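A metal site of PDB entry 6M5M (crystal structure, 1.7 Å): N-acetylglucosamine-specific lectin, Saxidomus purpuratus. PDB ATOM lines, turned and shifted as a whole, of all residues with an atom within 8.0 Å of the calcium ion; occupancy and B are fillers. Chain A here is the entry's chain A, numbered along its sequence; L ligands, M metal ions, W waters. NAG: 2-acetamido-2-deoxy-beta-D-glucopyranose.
An oxygen (O3) of the ligand is in hydrogen-bond range of a ring nitrogen (ND1) of His 140, at 2.8 Å.
The side-chain amide nitrogen (ND2) of Asn 138 is in hydrogen-bond range of an oxygen (O3) of the ligand (2.9 Å).
An oxygen (O6) of the ligand is in hydrogen-bond range of the guanidinium group (NH2) of Arg 117 (2.9 Å).
The side-chain carboxylate of Asp 126 lies close to an oxygen (O7) of the ligand (2.4 Å).
OD2 of Asp 139 lies close to N of Ala 120 (3.3 Å).
The backbone carbonyl oxygen of Ala 120 is in hydrogen-bond range of the side-chain amide nitrogen of Gln 141 (3.3 Å).
NE2 of Gln 141 lies within hydrogen-bond range of OH of Tyr 100, 3.2 Å away.
NE2 of Gln 141 lies close to N of Gly 123 (3.4 Å).
NE2 of Gln 141 is in hydrogen-bond range of O of Asp 121.
OD2 of Asp 119 is in salt-bridge range of NE of Arg 117, 3.3 Å away.
Within 4 Å of the calcium ion: Asp 119, Asp 139 and Gln 141.
The calcium ion is bound by water W2, at 2.2 Å.
O of Asp 139 binds the calcium ion (2.3 Å).
The calcium ion is bound by the side-chain amide oxygen (OE1) of Gln 141 (2.4 Å).
The calcium ion is bound by OD2 of Asp 139, at 2.4 Å.
Water W1 is bound to the calcium ion (2.4 Å).
Water W3 binds the calcium ion (2.4 Å).
OD1 of Asp 119 binds the calcium ion, 2.5 Å away.
Water W1 lies within hydrogen-bond range of the side-chain amide oxygen (OD1) of Asn 138, the side-chain carboxylate (OD2) of Asp 119, an oxygen (O4) of the ligand and the guanidinium group (NE) of Arg 117.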
ATOM      1  N   TYR A 100       7.351  22.647 -36.984  1.00  0.00           N
ATOM      2  CA  TYR A 100       6.331  21.682 -37.505  1.00  0.00           C
ATOM      3  C   TYR A 100       6.121  22.008 -38.980  1.00  0.00           C
ATOM      4  O   TYR A 100       5.993  23.189 -39.305  1.00  0.00           O
ATOM      5  CB  TYR A 100       5.050  21.665 -36.632  1.00  0.00           C
ATOM      6  CG  TYR A 100       5.292  21.048 -35.280  1.00  0.00           C
ATOM      7  CD1 TYR A 100       5.352  19.679 -35.119  1.00  0.00           C
ATOM      8  CD2 TYR A 100       5.650  21.827 -34.183  1.00  0.00           C
ATOM      9  CE1 TYR A 100       5.661  19.102 -33.903  1.00  0.00           C
ATOM     10  CE2 TYR A 100       5.991  21.266 -32.964  1.00  0.00           C
ATOM     11  CZ  TYR A 100       6.026  19.896 -32.829  1.00  0.00           C
ATOM     12  OH  TYR A 100       6.331  19.327 -31.618  1.00  0.00           O
ATOM     13  N   TRP A 113      -3.768  25.430 -34.872  1.00  0.00           N
ATOM     14  CA  TRP A 113      -3.336  24.990 -33.516  1.00  0.00           C
ATOM     15  C   TRP A 113      -4.368  25.366 -32.460  1.00  0.00           C
ATOM     16  O   TRP A 113      -4.961  26.449 -32.518  1.00  0.00           O
ATOM     17  CB  TRP A 113      -1.973  25.570 -33.122  1.00  0.00           C
ATOM     18  CG  TRP A 113      -0.876  25.116 -34.019  1.00  0.00           C
ATOM     19  CD1 TRP A 113      -0.378  25.777 -35.110  1.00  0.00           C
ATOM     20  CD2 TRP A 113      -0.144  23.886 -33.919  1.00  0.00           C
ATOM     21  NE1 TRP A 113       0.605  25.028 -35.693  1.00  0.00           N
ATOM     22  CE2 TRP A 113       0.792  23.871 -34.982  1.00  0.00           C
ATOM     23  CE3 TRP A 113      -0.177  22.797 -33.041  1.00  0.00           C
ATOM     24  CZ2 TRP A 113       1.683  22.827 -35.184  1.00  0.00           C
ATOM     25  CZ3 TRP A 113       0.692  21.744 -33.263  1.00  0.00           C
ATOM     26  CH2 TRP A 113       1.608  21.760 -34.320  1.00  0.00           C
ATOM     27  N   ASN A 116      -2.175  27.317 -27.122  1.00  0.00           N
ATOM     28  CA  ASN A 116      -0.821  27.083 -26.539  1.00  0.00           C
ATOM     29  C   ASN A 116      -0.176  25.854 -27.170  1.00  0.00           C
ATOM     30  O   ASN A 116       0.547  25.120 -26.475  1.00  0.00           O
ATOM     31  CB  ASN A 116      -0.852  26.995 -25.018  1.00  0.00           C
ATOM     32  CG  ASN A 116      -1.220  28.324 -24.415  1.00  0.00           C
ATOM     33  OD1 ASN A 116      -2.304  28.472 -23.845  1.00  0.00           O
ATOM     34  ND2 ASN A 116      -0.350  29.306 -24.591  1.00  0.00           N
ATOM     35  N   ARG A 117      -0.400  25.668 -28.465  1.00  0.00           N
ATOM     36  CA  ARG A 117       0.175  24.514 -29.190  1.00  0.00           C
ATOM     37  C   ARG A 117       0.918  25.035 -30.418  1.00  0.00           C
ATOM     38  O   ARG A 117       0.416  25.951 -31.037  1.00  0.00           O
ATOM     39  CB  ARG A 117      -0.925  23.515 -29.531  1.00  0.00           C
ATOM     40  CG  ARG A 117      -1.592  22.917 -28.303  1.00  0.00           C
ATOM     41  CD  ARG A 117      -0.636  22.093 -27.476  1.00  0.00           C
ATOM     42  NE  ARG A 117      -1.290  21.380 -26.395  1.00  0.00           N
ATOM     43  CZ  ARG A 117      -1.443  21.876 -25.186  1.00  0.00           C
ATOM     44  NH1 ARG A 117      -0.997  23.079 -24.916  1.00  0.00           N
ATOM     45  NH2 ARG A 117      -2.061  21.181 -24.255  1.00  0.00           N
ATOM     46  N   PRO A 118       2.098  24.492 -30.779  1.00  0.00           N
ATOM     47  CA  PRO A 118       2.691  23.331 -30.142  1.00  0.00           C
ATOM     48  C   PRO A 118       3.434  23.713 -28.856  1.00  0.00           C
ATOM     49  O   PRO A 118       4.024  24.748 -28.822  1.00  0.00           O
ATOM     50  CB  PRO A 118       3.707  22.900 -31.194  1.00  0.00           C
ATOM     51  CG  PRO A 118       4.215  24.197 -31.699  1.00  0.00           C
ATOM     52  CD  PRO A 118       2.952  25.020 -31.824  1.00  0.00           C
ATOM     53  N   ASP A 119       3.363  22.852 -27.853  1.00  0.00           N
ATOM     54  CA  ASP A 119       3.955  23.147 -26.511  1.00  0.00           C
ATOM     55  C   ASP A 119       5.340  22.526 -26.370  1.00  0.00           C
ATOM     56  O   ASP A 119       5.956  22.698 -25.305  1.00  0.00           O
ATOM     57  CB  ASP A 119       3.018  22.700 -25.387  1.00  0.00           C
ATOM     58  CG  ASP A 119       2.629  21.223 -25.443  1.00  0.00           C
ATOM     59  OD1 ASP A 119       3.358  20.447 -26.066  1.00  0.00           O
ATOM     60  OD2 ASP A 119       1.601  20.881 -24.866  1.00  0.00           O
ATOM     61  N   ALA A 120       5.845  21.862 -27.417  1.00  0.00           N
ATOM     62  CA  ALA A 120       7.175  21.216 -27.428  1.00  0.00           C
ATOM     63  C   ALA A 120       7.527  20.751 -28.852  1.00  0.00           C
ATOM     64  O   ALA A 120       6.612  20.503 -29.655  1.00  0.00           O
ATOM     65  CB  ALA A 120       7.204  20.048 -26.478  1.00  0.00           C
ATOM     66  N   ASP A 121       8.816  20.600 -29.113  1.00  0.00           N
ATOM     67  CA  ASP A 121       9.375  20.202 -30.433  1.00  0.00           C
ATOM     68  C   ASP A 121       9.392  18.664 -30.556  1.00  0.00           C
ATOM     69  O   ASP A 121       8.912  17.968 -29.629  1.00  0.00           O
ATOM     70  CB  ASP A 121      10.769  20.826 -30.597  1.00  0.00           C
ATOM     71  CG  ASP A 121      10.810  22.302 -30.195  1.00  0.00           C
ATOM     72  OD1 ASP A 121      10.063  23.112 -30.780  1.00  0.00           O
ATOM     73  OD2 ASP A 121      11.573  22.617 -29.282  1.00  0.00           O
ATOM     74  N   GLU A 122       9.918  18.159 -31.670  1.00  0.00           N
ATOM     75  CA  GLU A 122      10.042  16.707 -31.966  1.00  0.00           C
ATOM     76  C   GLU A 122       8.741  15.957 -31.622  1.00  0.00           C
ATOM     77  O   GLU A 122       8.818  14.859 -31.001  1.00  0.00           O
ATOM     78  CB  GLU A 122      11.246  16.149 -31.200  1.00  0.00           C
ATOM     79  CG  GLU A 122      12.555  16.767 -31.650  1.00  0.00           C
ATOM     80  CD  GLU A 122      13.692  16.586 -30.648  1.00  0.00           C
ATOM     81  OE1 GLU A 122      13.482  16.877 -29.449  1.00  0.00           O
ATOM     82  OE2 GLU A 122      14.771  16.142 -31.078  1.00  0.00           O
ATOM     83  N   GLY A 123       7.588  16.520 -32.008  1.00  0.00           N
ATOM     84  CA  GLY A 123       6.294  15.813 -31.919  1.00  0.00           C
ATOM     85  C   GLY A 123       5.718  15.488 -33.284  1.00  0.00           C
ATOM     86  O   GLY A 123       6.369  15.752 -34.280  1.00  0.00           O
ATOM     87  N   CYS A 124       4.558  14.859 -33.297  1.00  0.00           N
ATOM     88  CA  CYS A 124       3.676  14.651 -34.470  1.00  0.00           C
ATOM     89  C   CYS A 124       2.329  15.271 -34.102  1.00  0.00           C
ATOM     90  O   CYS A 124       2.061  15.399 -32.901  1.00  0.00           O
ATOM     91  CB  CYS A 124       3.515  13.184 -34.824  1.00  0.00           C
ATOM     92  SG  CYS A 124       3.469  12.099 -33.386  1.00  0.00           S
ATOM     93  N   ASP A 126      -1.931  15.829 -34.140  1.00  0.00           N
ATOM     94  CA  ASP A 126      -3.235  15.152 -34.165  1.00  0.00           C
ATOM     95  C   ASP A 126      -4.332  16.200 -33.944  1.00  0.00           C
ATOM     96  O   ASP A 126      -4.018  17.275 -33.465  1.00  0.00           O
ATOM     97  CB  ASP A 126      -3.340  14.070 -33.087  1.00  0.00           C
ATOM     98  CG  ASP A 126      -3.053  14.504 -31.670  1.00  0.00           C
ATOM     99  OD1 ASP A 126      -2.702  15.633 -31.473  1.00  0.00           O
ATOM    100  OD2 ASP A 126      -3.191  13.682 -30.781  1.00  0.00           O
ATOM    101  N   ASN A 138      -2.861  19.528 -31.953  1.00  0.00           N
ATOM    102  CA  ASN A 138      -1.945  19.388 -30.809  1.00  0.00           C
ATOM    103  C   ASN A 138      -0.693  18.656 -31.319  1.00  0.00           C
ATOM    104  O   ASN A 138      -0.776  18.015 -32.352  1.00  0.00           O
ATOM    105  CB  ASN A 138      -2.647  18.685 -29.649  1.00  0.00           C
ATOM    106  CG  ASN A 138      -1.737  18.197 -28.546  1.00  0.00           C
ATOM    107  OD1 ASN A 138      -1.330  18.975 -27.685  1.00  0.00           O
ATOM    108  ND2 ASN A 138      -1.421  16.898 -28.576  1.00  0.00           N
ATOM    109  N   ASP A 139       0.422  18.864 -30.638  1.00  0.00           N
ATOM    110  CA  ASP A 139       1.694  18.122 -30.813  1.00  0.00           C
ATOM    111  C   ASP A 139       1.806  17.109 -29.680  1.00  0.00           C
ATOM    112  O   ASP A 139       1.602  17.515 -28.501  1.00  0.00           O
ATOM    113  CB  ASP A 139       2.893  19.073 -30.767  1.00  0.00           C
ATOM    114  CG  ASP A 139       3.050  19.792 -29.439  1.00  0.00           C
ATOM    115  OD1 ASP A 139       2.203  20.672 -29.147  1.00  0.00           O
ATOM    116  OD2 ASP A 139       3.964  19.403 -28.685  1.00  0.00           O
ATOM    117  N   HIS A 140       2.058  15.855 -30.037  1.00  0.00           N
ATOM    118  CA  HIS A 140       2.319  14.703 -29.138  1.00  0.00           C
ATOM    119  C   HIS A 140       3.786  14.282 -29.320  1.00  0.00           C
ATOM    120  O   HIS A 140       4.185  14.202 -30.478  1.00  0.00           O
ATOM    121  CB  HIS A 140       1.353  13.524 -29.468  1.00  0.00           C
ATOM    122  CG  HIS A 140       1.286  12.533 -28.347  1.00  0.00           C
ATOM    123  ND1 HIS A 140       0.824  12.925 -27.071  1.00  0.00           N
ATOM    124  CD2 HIS A 140       1.651  11.247 -28.243  1.00  0.00           C
ATOM    125  CE1 HIS A 140       0.922  11.905 -26.266  1.00  0.00           C
ATOM    126  NE2 HIS A 140       1.364  10.849 -26.951  1.00  0.00           N
ATOM    127  N   GLN A 141       4.501  13.929 -28.258  1.00  0.00           N
ATOM    128  CA  GLN A 141       5.965  13.618 -28.354  1.00  0.00           C
ATOM    129  C   GLN A 141       6.224  12.107 -28.406  1.00  0.00           C
ATOM    130  O   GLN A 141       7.400  11.722 -28.400  1.00  0.00           O
ATOM    131  CB  GLN A 141       6.720  14.309 -27.231  1.00  0.00           C
ATOM    132  CG  GLN A 141       7.113  15.758 -27.553  1.00  0.00           C
ATOM    133  CD  GLN A 141       5.953  16.618 -27.978  1.00  0.00           C
ATOM    134  OE1 GLN A 141       4.955  16.723 -27.272  1.00  0.00           O
ATOM    135  NE2 GLN A 141       6.098  17.315 -29.088  1.00  0.00           N
ATOM    136  N   ASP A 142       5.181  11.265 -28.519  1.00  0.00           N
ATOM    137  CA  ASP A 142       5.331   9.808 -28.802  1.00  0.00           C
ATOM    138  C   ASP A 142       4.701   9.526 -30.155  1.00  0.00           C
ATOM    139  O   ASP A 142       3.418   9.354 -30.268  1.00  0.00           O
ATOM    140  CB  ASP A 142       4.765   8.893 -27.710  1.00  0.00           C
ATOM    141  CG  ASP A 142       4.934   7.405 -27.998  1.00  0.00           C
ATOM    142  OD1 ASP A 142       5.451   7.034 -29.064  1.00  0.00           O
ATOM    143  OD2 ASP A 142       4.542   6.598 -27.141  1.00  0.00           O
HETATM  144  C1  NAG L   1      -3.102  14.648 -24.277  1.00  0.00           C
HETATM  145  C2  NAG L   1      -2.622  14.571 -25.710  1.00  0.00           C
HETATM  146  C3  NAG L   1      -1.273  15.204 -25.321  1.00  0.00           C
HETATM  147  C4  NAG L   1      -1.543  16.548 -24.749  1.00  0.00           C
HETATM  148  C5  NAG L   1      -2.618  16.577 -23.658  1.00  0.00           C
HETATM  149  C6  NAG L   1      -2.881  18.003 -23.273  1.00  0.00           C
HETATM  150  C7  NAG L   1      -2.595  13.016 -27.565  1.00  0.00           C
HETATM  151  C8  NAG L   1      -2.440  11.620 -27.919  1.00  0.00           C
HETATM  152  N2  NAG L   1      -2.563  13.237 -26.226  1.00  0.00           N
HETATM  153  O1  NAG L   1      -3.479  13.513 -23.614  1.00  0.00           O
HETATM  154  O3  NAG L   1      -0.365  15.352 -26.402  1.00  0.00           O
HETATM  155  O4  NAG L   1      -0.352  17.152 -24.175  1.00  0.00           O
HETATM  156  O5  NAG L   1      -3.792  15.848 -24.116  1.00  0.00           O
HETATM  157  O6  NAG L   1      -3.541  18.641 -24.337  1.00  0.00           O
HETATM  158  O7  NAG L   1      -2.747  13.882 -28.423  1.00  0.00           O
HETATM  159 CA    CA M   1       3.089  18.119 -26.840  1.00  0.00          CA
HETATM  160  O   HOH W   1       0.819  18.624 -26.125  1.00  0.00           O
HETATM  161  O   HOH W   2       4.416  18.326 -25.072  1.00  0.00           O
HETATM  162  O   HOH W   3       2.436  15.958 -25.907  1.00  0.00           O
